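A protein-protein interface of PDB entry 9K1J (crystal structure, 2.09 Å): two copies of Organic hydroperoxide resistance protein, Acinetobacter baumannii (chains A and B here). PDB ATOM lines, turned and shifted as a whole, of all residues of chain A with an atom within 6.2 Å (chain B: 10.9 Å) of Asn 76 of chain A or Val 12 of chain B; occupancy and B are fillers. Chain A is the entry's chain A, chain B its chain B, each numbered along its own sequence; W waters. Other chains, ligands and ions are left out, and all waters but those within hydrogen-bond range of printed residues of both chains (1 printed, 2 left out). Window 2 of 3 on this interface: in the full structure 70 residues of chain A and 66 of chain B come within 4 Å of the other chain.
Water W1 lies within hydrogen-bond range of OE2 of Glu 79 of chain A (2.4 Å) and NZ of Lys 10 of chain B (3.2 Å).
The backbone NH of Gly 13 of chain B sits at hydrogen-bond distance from the backbone carbonyl oxygen of Val 78 of chain A, at 3.2 Å. N of Ala 11 of chain B is in hydrogen-bond range of O of Val 80 of chain A (2.7 Å).
No position is printed for both chains. Of the 10 pairs that touch across the chains among the printed residues, none has its exchanged pair printed and touching as well.
Among the printed residues, merely in contact across the chains: Val 80 of chain A with Lys 10 of chain B (3.4 Å), Asp 75 of chain A with Gly 13 of chain B (3.4 Å), Glu 79 of chain A with Ala 11 of chain B (3.5 Å), Glu 79 of chain A with Lys 10 of chain B (3.5 Å), Val 78 of chain A with Val 12 of chain B (3.6 Å), Val 80 of chain A with Val 9 of chain B (3.6 Å), Asn 76 of chain A with Val 12 of chain B (3.7 Å) and Ile 62 of chain A with Gly 13 of chain B (3.9 Å).
Of the 9 printed residues of chain A, 6 touch a printed residue of chain B. Printed residues of chain A that touch a printed residue of chain B: Ile 62, Asp 75, Asn 76, Val 78, Glu 79 and Val 80. Hydrophobic or aromatic side chains of chain B within 4 Å of the printed part of chain A: Ala 11 and Val 12.
Asn 76 of chain A touches just one residue of chain B: Val 12 (3.7 Å). Printed residues of chain A within 4 Å of Val 12 of chain B: Asn 76 (3.7 Å) and Val 78 (3.6 Å). Of chain B, only Gly 13 (3.4 Å) comes within 4 Å of Asp 75 of chain A. No residue of chain B comes within 4 Å of Asp 77 of chain A. Printed residues of chain B within 4 Å of Val 78 of chain A: Val 12 (3.6 Å) and Gly 13 (3.2 Å). Of the printed residues of chain B, Glu 79 of chain A touches Lys 10 and Ala 11. Of the printed residues of chain A, Ala 11 of chain B touches Glu 79 (3.5 Å) and Val 80 (2.7 Å). Printed residues of chain B within 4 Å of Val 80 of chain A: Val 9 (3.6 Å), Lys 10 (3.4 Å) and Ala 11 (2.7 Å). Ile 19 of chain B touches none of the printed residues of chain A. Glu 22 of chain B touches none of the printed residues of chain A.
O of Arg 20 of chain B sits at hydrogen-bond distance from N of Lys 10 of chain B (2.9 Å). NZ of Lys 10 of chain B is in salt-bridge range of OE2 of Glu 22 of chain B (3.9 Å). N of Thr 18 of chain B lies within hydrogen-bond range of O of Val 12 of chain B, at 2.9 Å.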
ATOM      1  N   ILE A  62       6.411  -2.899 -23.133  1.00  0.00           N
ATOM      2  CA  ILE A  62       6.305  -1.443 -23.042  1.00  0.00           C
ATOM      3  C   ILE A  62       7.636  -0.804 -23.402  1.00  0.00           C
ATOM      4  O   ILE A  62       7.703   0.131 -24.215  1.00  0.00           O
ATOM      5  CB  ILE A  62       5.849  -1.004 -21.637  1.00  0.00           C
ATOM      6  CG1 ILE A  62       4.392  -1.364 -21.384  1.00  0.00           C
ATOM      7  CG2 ILE A  62       6.066   0.491 -21.426  1.00  0.00           C
ATOM      8  CD1 ILE A  62       4.032  -1.350 -19.913  1.00  0.00           C
ATOM      9  N   ARG A  74       0.549   4.087 -23.794  1.00  0.00           N
ATOM     10  CA  ARG A  74       0.528   4.080 -22.339  1.00  0.00           C
ATOM     11  C   ARG A  74       0.387   2.676 -21.756  1.00  0.00           C
ATOM     12  O   ARG A  74      -0.085   1.741 -22.412  1.00  0.00           O
ATOM     13  CB  ARG A  74      -0.560   5.016 -21.818  1.00  0.00           C
ATOM     14  CG  ARG A  74      -1.942   4.789 -22.349  1.00  0.00           C
ATOM     15  CD  ARG A  74      -2.760   5.908 -21.717  1.00  0.00           C
ATOM     16  NE  ARG A  74      -4.092   6.081 -22.265  1.00  0.00           N
ATOM     17  CZ  ARG A  74      -4.975   6.955 -21.778  1.00  0.00           C
ATOM     18  NH1 ARG A  74      -4.695   7.658 -20.669  1.00  0.00           N
ATOM     19  NH2 ARG A  74      -6.172   7.082 -22.356  1.00  0.00           N
ATOM     20  N   ASP A  75       0.851   2.561 -20.502  1.00  0.00           N
ATOM     21  CA  ASP A  75       1.052   1.288 -19.818  1.00  0.00           C
ATOM     22  C   ASP A  75      -0.073   0.302 -20.087  1.00  0.00           C
ATOM     23  O   ASP A  75       0.156  -0.822 -20.550  1.00  0.00           O
ATOM     24  CB  ASP A  75       1.191   1.513 -18.300  1.00  0.00           C
ATOM     25  CG  ASP A  75       2.552   2.090 -17.896  1.00  0.00           C
ATOM     26  OD1 ASP A  75       3.397   2.333 -18.791  1.00  0.00           O
ATOM     27  OD2 ASP A  75       2.769   2.287 -16.671  1.00  0.00           O
ATOM     28  N   ASN A  76      -1.301   0.730 -19.840  1.00  0.00           N
ATOM     29  CA  ASN A  76      -2.414  -0.196 -19.924  1.00  0.00           C
ATOM     30  C   ASN A  76      -2.797  -0.548 -21.357  1.00  0.00           C
ATOM     31  O   ASN A  76      -3.764  -1.297 -21.539  1.00  0.00           O
ATOM     32  CB  ASN A  76      -3.591   0.389 -19.154  1.00  0.00           C
ATOM     33  CG  ASN A  76      -3.201   0.761 -17.738  1.00  0.00           C
ATOM     34  OD1 ASN A  76      -3.144  -0.091 -16.850  1.00  0.00           O
ATOM     35  ND2 ASN A  76      -2.862   2.034 -17.538  1.00  0.00           N
ATOM     36  N   ASP A  77      -2.059  -0.075 -22.367  1.00  0.00           N
ATOM     37  CA  ASP A  77      -2.261  -0.551 -23.731  1.00  0.00           C
ATOM     38  C   ASP A  77      -1.594  -1.898 -23.983  1.00  0.00           C
ATOM     39  O   ASP A  77      -1.554  -2.346 -25.139  1.00  0.00           O
ATOM     40  CB  ASP A  77      -1.741   0.477 -24.743  1.00  0.00           C
ATOM     41  CG  ASP A  77      -2.480   1.816 -24.662  1.00  0.00           C
ATOM     42  OD1 ASP A  77      -3.668   1.835 -24.259  1.00  0.00           O
ATOM     43  OD2 ASP A  77      -1.873   2.858 -25.022  1.00  0.00           O
ATOM     44  N   VAL A  78      -1.057  -2.533 -22.940  1.00  0.00           N
ATOM     45  CA  VAL A  78      -0.380  -3.819 -23.036  1.00  0.00           C
ATOM     46  C   VAL A  78      -1.020  -4.765 -22.036  1.00  0.00           C
ATOM     47  O   VAL A  78      -1.007  -4.508 -20.827  1.00  0.00           O
ATOM     48  CB  VAL A  78       1.126  -3.715 -22.760  1.00  0.00           C
ATOM     49  CG1 VAL A  78       1.773  -5.088 -22.970  1.00  0.00           C
ATOM     50  CG2 VAL A  78       1.764  -2.674 -23.644  1.00  0.00           C
ATOM     51  N   GLU A  79      -1.566  -5.856 -22.538  1.00  0.00           N
ATOM     52  CA  GLU A  79      -2.070  -6.938 -21.711  1.00  0.00           C
ATOM     53  C   GLU A  79      -1.331  -8.208 -22.090  1.00  0.00           C
ATOM     54  O   GLU A  79      -1.097  -8.459 -23.272  1.00  0.00           O
ATOM     55  CB  GLU A  79      -3.566  -7.135 -21.911  1.00  0.00           C
ATOM     56  CG  GLU A  79      -4.102  -8.340 -21.171  1.00  0.00           C
ATOM     57  CD  GLU A  79      -5.482  -8.739 -21.645  1.00  0.00           C
ATOM     58  OE1 GLU A  79      -5.701  -9.955 -21.920  1.00  0.00           O
ATOM     59  OE2 GLU A  79      -6.351  -7.830 -21.725  1.00  0.00           O
ATOM     60  N   VAL A  80      -0.936  -8.991 -21.093  1.00  0.00           N
ATOM     61  CA  VAL A  80      -0.364 -10.313 -21.321  1.00  0.00           C
ATOM     62  C   VAL A  80      -1.198 -11.309 -20.529  1.00  0.00           C
ATOM     63  O   VAL A  80      -1.399 -11.143 -19.321  1.00  0.00           O
ATOM     64  CB  VAL A  80       1.118 -10.392 -20.914  1.00  0.00           C
ATOM     65  CG1 VAL A  80       1.646 -11.826 -21.117  1.00  0.00           C
ATOM     66  CG2 VAL A  80       1.933  -9.405 -21.708  1.00  0.00           C
ATOM     67  N   SER A 105      -2.761  -2.439 -27.686  1.00  0.00           N
ATOM     68  CA  SER A 105      -3.774  -1.517 -28.184  1.00  0.00           C
ATOM     69  C   SER A 105      -3.128  -0.429 -29.030  1.00  0.00           C
ATOM     70  O   SER A 105      -2.111   0.150 -28.638  1.00  0.00           O
ATOM     71  CB  SER A 105      -4.550  -0.874 -27.031  1.00  0.00           C
ATOM     72  OG  SER A 105      -5.285  -1.846 -26.322  1.00  0.00           O
ATOM     73  N   VAL B   9      -3.275 -16.279 -16.042  1.00  0.00           N
ATOM     74  CA  VAL B   9      -3.137 -15.043 -15.284  1.00  0.00           C
ATOM     75  C   VAL B   9      -2.981 -13.896 -16.270  1.00  0.00           C
ATOM     76  O   VAL B   9      -2.136 -13.955 -17.176  1.00  0.00           O
ATOM     77  CB  VAL B   9      -1.944 -15.058 -14.307  1.00  0.00           C
ATOM     78  CG1 VAL B   9      -1.862 -13.709 -13.580  1.00  0.00           C
ATOM     79  CG2 VAL B   9      -2.053 -16.213 -13.298  1.00  0.00           C
ATOM     80  N   LYS B  10      -3.787 -12.848 -16.082  1.00  0.00           N
ATOM     81  CA  LYS B  10      -3.783 -11.674 -16.945  1.00  0.00           C
ATOM     82  C   LYS B  10      -3.020 -10.567 -16.232  1.00  0.00           C
ATOM     83  O   LYS B  10      -3.349 -10.227 -15.092  1.00  0.00           O
ATOM     84  CB  LYS B  10      -5.220 -11.238 -17.253  1.00  0.00           C
ATOM     85  CG  LYS B  10      -5.320 -10.045 -18.200  1.00  0.00           C
ATOM     86  CD  LYS B  10      -6.752  -9.581 -18.453  1.00  0.00           C
ATOM     87  CE  LYS B  10      -7.674 -10.692 -18.929  1.00  0.00           C
ATOM     88  NZ  LYS B  10      -9.052 -10.161 -19.237  1.00  0.00           N
ATOM     89  N   ALA B  11      -1.992 -10.027 -16.886  1.00  0.00           N
ATOM     90  CA  ALA B  11      -1.220  -8.908 -16.360  1.00  0.00           C
ATOM     91  C   ALA B  11      -1.375  -7.705 -17.286  1.00  0.00           C
ATOM     92  O   ALA B  11      -1.138  -7.813 -18.498  1.00  0.00           O
ATOM     93  CB  ALA B  11       0.255  -9.273 -16.209  1.00  0.00           C
ATOM     94  N   VAL B  12      -1.745  -6.560 -16.709  1.00  0.00           N
ATOM     95  CA  VAL B  12      -1.970  -5.326 -17.458  1.00  0.00           C
ATOM     96  C   VAL B  12      -1.032  -4.236 -16.946  1.00  0.00           C
ATOM     97  O   VAL B  12      -0.998  -3.957 -15.738  1.00  0.00           O
ATOM     98  CB  VAL B  12      -3.435  -4.862 -17.345  1.00  0.00           C
ATOM     99  CG1 VAL B  12      -3.622  -3.548 -18.090  1.00  0.00           C
ATOM    100  CG2 VAL B  12      -4.359  -5.937 -17.884  1.00  0.00           C
ATOM    101  N   GLY B  13      -0.297  -3.601 -17.864  1.00  0.00           N
ATOM    102  CA  GLY B  13       0.457  -2.405 -17.525  1.00  0.00           C
ATOM    103  C   GLY B  13       1.837  -2.641 -16.951  1.00  0.00           C
ATOM    104  O   GLY B  13       2.382  -1.741 -16.291  1.00  0.00           O
ATOM    105  N   GLY B  14       2.412  -3.827 -17.162  1.00  0.00           N
ATOM    106  CA  GLY B  14       3.795  -4.077 -16.772  1.00  0.00           C
ATOM    107  C   GLY B  14       4.045  -3.988 -15.275  1.00  0.00           C
ATOM    108  O   GLY B  14       3.194  -4.336 -14.439  1.00  0.00           O
ATOM    109  N   ARG B  15       5.247  -3.525 -14.924  1.00  0.00           N
ATOM    110  CA  ARG B  15       5.687  -3.560 -13.534  1.00  0.00           C
ATOM    111  C   ARG B  15       4.998  -2.523 -12.653  1.00  0.00           C
ATOM    112  O   ARG B  15       5.148  -2.592 -11.426  1.00  0.00           O
ATOM    113  CB  ARG B  15       7.205  -3.377 -13.474  1.00  0.00           C
ATOM    114  CG  ARG B  15       7.947  -4.670 -13.789  1.00  0.00           C
ATOM    115  CD  ARG B  15       9.414  -4.432 -13.969  1.00  0.00           C
ATOM    116  NE  ARG B  15      10.079  -5.652 -14.420  1.00  0.00           N
ATOM    117  CZ  ARG B  15      10.734  -6.484 -13.631  1.00  0.00           C
ATOM    118  NH1 ARG B  15      10.846  -6.217 -12.337  1.00  0.00           N
ATOM    119  NH2 ARG B  15      11.311  -7.555 -14.149  1.00  0.00           N
ATOM    120  N   SER B  16       4.240  -1.585 -13.231  1.00  0.00           N
ATOM    121  CA  SER B  16       3.425  -0.664 -12.446  1.00  0.00           C
ATOM    122  C   SER B  16       1.935  -0.980 -12.517  1.00  0.00           C
ATOM    123  O   SER B  16       1.126  -0.170 -12.060  1.00  0.00           O
ATOM    124  CB  SER B  16       3.658   0.785 -12.890  1.00  0.00           C
ATOM    125  OG  SER B  16       4.848   1.312 -12.323  1.00  0.00           O
ATOM    126  N   GLY B  17       1.552  -2.138 -13.054  1.00  0.00           N
ATOM    127  CA  GLY B  17       0.153  -2.451 -13.285  1.00  0.00           C
ATOM    128  C   GLY B  17      -0.470  -3.445 -12.328  1.00  0.00           C
ATOM    129  O   GLY B  17      -0.375  -3.277 -11.112  1.00  0.00           O
ATOM    130  N   THR B  18      -1.144  -4.471 -12.856  1.00  0.00           N
ATOM    131  CA  THR B  18      -1.915  -5.403 -12.039  1.00  0.00           C
ATOM    132  C   THR B  18      -1.786  -6.814 -12.612  1.00  0.00           C
ATOM    133  O   THR B  18      -1.462  -6.999 -13.792  1.00  0.00           O
ATOM    134  CB  THR B  18      -3.400  -5.030 -11.988  1.00  0.00           C
ATOM    135  OG1 THR B  18      -3.939  -5.073 -13.318  1.00  0.00           O
ATOM    136  CG2 THR B  18      -3.600  -3.626 -11.426  1.00  0.00           C
ATOM    137  N   ILE B  19      -2.040  -7.812 -11.759  1.00  0.00           N
ATOM    138  CA  ILE B  19      -2.178  -9.204 -12.180  1.00  0.00           C
ATOM    139  C   ILE B  19      -3.463  -9.743 -11.582  1.00  0.00           C
ATOM    140  O   ILE B  19      -3.850  -9.376 -10.465  1.00  0.00           O
ATOM    141  CB  ILE B  19      -1.015 -10.124 -11.734  1.00  0.00           C
ATOM    142  CG1 ILE B  19      -0.962 -10.135 -10.198  1.00  0.00           C
ATOM    143  CG2 ILE B  19       0.277  -9.684 -12.333  1.00  0.00           C
ATOM    144  CD1 ILE B  19      -0.109 -11.183  -9.604  1.00  0.00           C
ATOM    145  N   ARG B  20      -4.081 -10.680 -12.298  1.00  0.00           N
ATOM    146  CA  ARG B  20      -5.271 -11.335 -11.776  1.00  0.00           C
ATOM    147  C   ARG B  20      -5.456 -12.665 -12.485  1.00  0.00           C
ATOM    148  O   ARG B  20      -5.455 -12.713 -13.716  1.00  0.00           O
ATOM    149  CB  ARG B  20      -6.509 -10.434 -11.946  1.00  0.00           C
ATOM    150  CG  ARG B  20      -7.783 -11.077 -11.488  1.00  0.00           C
ATOM    151  CD  ARG B  20      -9.004 -10.323 -12.000  1.00  0.00           C
ATOM    152  NE  ARG B  20     -10.200 -10.887 -11.392  1.00  0.00           N
ATOM    153  CZ  ARG B  20     -10.865 -11.929 -11.868  1.00  0.00           C
ATOM    154  NH1 ARG B  20     -10.489 -12.514 -13.008  1.00  0.00           N
ATOM    155  NH2 ARG B  20     -11.923 -12.378 -11.208  1.00  0.00           N
ATOM    156  N   SER B  21      -5.591 -13.738 -11.716  1.00  0.00           N
ATOM    157  CA  SER B  21      -5.869 -15.025 -12.326  1.00  0.00           C
ATOM    158  C   SER B  21      -7.310 -15.060 -12.826  1.00  0.00           C
ATOM    159  O   SER B  21      -8.191 -14.347 -12.327  1.00  0.00           O
ATOM    160  CB  SER B  21      -5.612 -16.159 -11.332  1.00  0.00           C
ATOM    161  OG  SER B  21      -6.219 -15.892 -10.082  1.00  0.00           O
ATOM    162  N   GLU B  22      -7.542 -15.889 -13.840  1.00  0.00           N
ATOM    163  CA  GLU B  22      -8.864 -15.950 -14.449  1.00  0.00           C
ATOM    164  C   GLU B  22      -9.888 -16.584 -13.515  1.00  0.00           C
ATOM    165  O   GLU B  22     -11.091 -16.409 -13.731  1.00  0.00           O
ATOM    166  CB  GLU B  22      -8.790 -16.713 -15.774  1.00  0.00           C
ATOM    167  CG  GLU B  22      -8.234 -15.901 -16.953  1.00  0.00           C
ATOM    168  CD  GLU B  22      -9.073 -14.664 -17.314  1.00  0.00           C
ATOM    169  OE1 GLU B  22     -10.299 -14.785 -17.521  1.00  0.00           O
ATOM    170  OE2 GLU B  22      -8.497 -13.563 -17.395  1.00  0.00           O
ATOM    171  N   LEU B  26      -5.921 -15.339  -7.335  1.00  0.00           N
ATOM    172  CA  LEU B  26      -4.774 -14.444  -7.166  1.00  0.00           C
ATOM    173  C   LEU B  26      -5.052 -13.132  -7.888  1.00  0.00           C
ATOM    174  O   LEU B  26      -5.277 -13.125  -9.099  1.00  0.00           O
ATOM    175  CB  LEU B  26      -3.479 -15.085  -7.681  1.00  0.00           C
ATOM    176  CG  LEU B  26      -2.228 -14.197  -7.640  1.00  0.00           C
ATOM    177  CD1 LEU B  26      -1.747 -14.038  -6.200  1.00  0.00           C
ATOM    178  CD2 LEU B  26      -1.114 -14.819  -8.518  1.00  0.00           C
ATOM    179  N   GLU B  27      -5.023 -12.026  -7.151  1.00  0.00           N
ATOM    180  CA  GLU B  27      -5.365 -10.715  -7.698  1.00  0.00           C
ATOM    181  C   GLU B  27      -4.565  -9.675  -6.930  1.00  0.00           C
ATOM    182  O   GLU B  27      -4.784  -9.494  -5.729  1.00  0.00           O
ATOM    183  CB  GLU B  27      -6.878 -10.460  -7.574  1.00  0.00           C
ATOM    184  CG  GLU B  27      -7.315  -8.998  -7.734  1.00  0.00           C
ATOM    185  CD  GLU B  27      -8.835  -8.832  -7.936  1.00  0.00           C
ATOM    186  OE1 GLU B  27      -9.358  -7.717  -7.705  1.00  0.00           O
ATOM    187  OE2 GLU B  27      -9.501  -9.809  -8.343  1.00  0.00           O
ATOM    188  N   LEU B  28      -3.624  -9.020  -7.602  1.00  0.00           N
ATOM    189  CA  LEU B  28      -2.660  -8.209  -6.879  1.00  0.00           C
ATOM    190  C   LEU B  28      -2.267  -7.024  -7.731  1.00  0.00           C
ATOM    191  O   LEU B  28      -2.272  -7.096  -8.956  1.00  0.00           O
ATOM    192  CB  LEU B  28      -1.402  -9.009  -6.516  1.00  0.00           C
ATOM    193  CG  LEU B  28      -1.428 -10.202  -5.544  1.00  0.00           C
ATOM    194  CD1 LEU B  28      -0.027 -10.819  -5.523  1.00  0.00           C
ATOM    195  CD2 LEU B  28      -1.882  -9.827  -4.141  1.00  0.00           C
ATOM    196  N   LYS B  29      -1.850  -5.962  -7.076  1.00  0.00           N
ATOM    197  CA  LYS B  29      -1.221  -4.869  -7.792  1.00  0.00           C
ATOM    198  C   LYS B  29       0.292  -4.927  -7.596  1.00  0.00           C
ATOM    199  O   LYS B  29       0.794  -5.544  -6.646  1.00  0.00           O
ATOM    200  CB  LYS B  29      -1.822  -3.551  -7.314  1.00  0.00           C
ATOM    201  CG  LYS B  29      -1.310  -2.261  -7.928  1.00  0.00           C
ATOM    202  CD  LYS B  29      -0.229  -1.741  -7.033  1.00  0.00           C
ATOM    203  CE  LYS B  29      -0.887  -1.318  -5.726  1.00  0.00           C
ATOM    204  NZ  LYS B  29       0.080  -0.780  -4.729  1.00  0.00           N
ATOM    205  N   LEU B  30       1.016  -4.338  -8.551  1.00  0.00           N
ATOM    206  CA  LEU B  30       2.470  -4.394  -8.606  1.00  0.00           C
ATOM    207  C   LEU B  30       3.055  -2.993  -8.553  1.00  0.00           C
ATOM    208  O   LEU B  30       2.433  -2.027  -8.993  1.00  0.00           O
ATOM    209  CB  LEU B  30       2.955  -5.072  -9.895  1.00  0.00           C
ATOM    210  CG  LEU B  30       2.399  -6.469 -10.197  1.00  0.00           C
ATOM    211  CD1 LEU B  30       3.005  -7.007 -11.479  1.00  0.00           C
ATOM    212  CD2 LEU B  30       2.627  -7.409  -9.061  1.00  0.00           C
ATOM    213  N   ALA B  31       4.272  -2.898  -8.039  1.00  0.00           N
ATOM    214  CA  ALA B  31       4.983  -1.636  -7.999  1.00  0.00           C
ATOM    215  C   ALA B  31       6.463  -1.916  -8.201  1.00  0.00           C
ATOM    216  O   ALA B  31       6.979  -2.927  -7.711  1.00  0.00           O
ATOM    217  CB  ALA B  31       4.752  -0.893  -6.674  1.00  0.00           C
ATOM    218  N   THR B  43       3.984  -5.901  -4.624  1.00  0.00           N
ATOM    219  CA  THR B  43       4.913  -6.924  -5.046  1.00  0.00           C
ATOM    220  C   THR B  43       5.362  -6.650  -6.485  1.00  0.00           C
ATOM    221  O   THR B  43       5.068  -5.604  -7.072  1.00  0.00           O
ATOM    222  CB  THR B  43       4.276  -8.300  -4.860  1.00  0.00           C
ATOM    223  OG1 THR B  43       5.274  -9.303  -5.053  1.00  0.00           O
ATOM    224  CG2 THR B  43       3.123  -8.513  -5.853  1.00  0.00           C
ATOM    225  N   PRO B  45       7.600  -8.830 -10.135  1.00  0.00           N
ATOM    226  CA  PRO B  45       7.850 -10.132 -10.772  1.00  0.00           C
ATOM    227  C   PRO B  45       8.903 -10.999 -10.091  1.00  0.00           C
ATOM    228  O   PRO B  45       8.806 -12.240 -10.146  1.00  0.00           O
ATOM    229  CB  PRO B  45       8.301  -9.717 -12.180  1.00  0.00           C
ATOM    230  CG  PRO B  45       7.442  -8.508 -12.441  1.00  0.00           C
ATOM    231  CD  PRO B  45       7.629  -7.747 -11.139  1.00  0.00           C
ATOM    232  N   LEU B  48       7.318 -12.521  -6.962  1.00  0.00           N
ATOM    233  CA  LEU B  48       6.368 -13.568  -7.338  1.00  0.00           C
ATOM    234  C   LEU B  48       7.085 -14.828  -7.824  1.00  0.00           C
ATOM    235  O   LEU B  48       6.707 -15.947  -7.442  1.00  0.00           O
ATOM    236  CB  LEU B  48       5.415 -13.048  -8.417  1.00  0.00           C
ATOM    237  CG  LEU B  48       4.303 -12.080  -8.002  1.00  0.00           C
ATOM    238  CD1 LEU B  48       3.752 -11.406  -9.258  1.00  0.00           C
ATOM    239  CD2 LEU B  48       3.188 -12.773  -7.185  1.00  0.00           C
HETATM  240  O   HOH W   1      -8.746  -8.007 -21.641  1.00  0.00           O
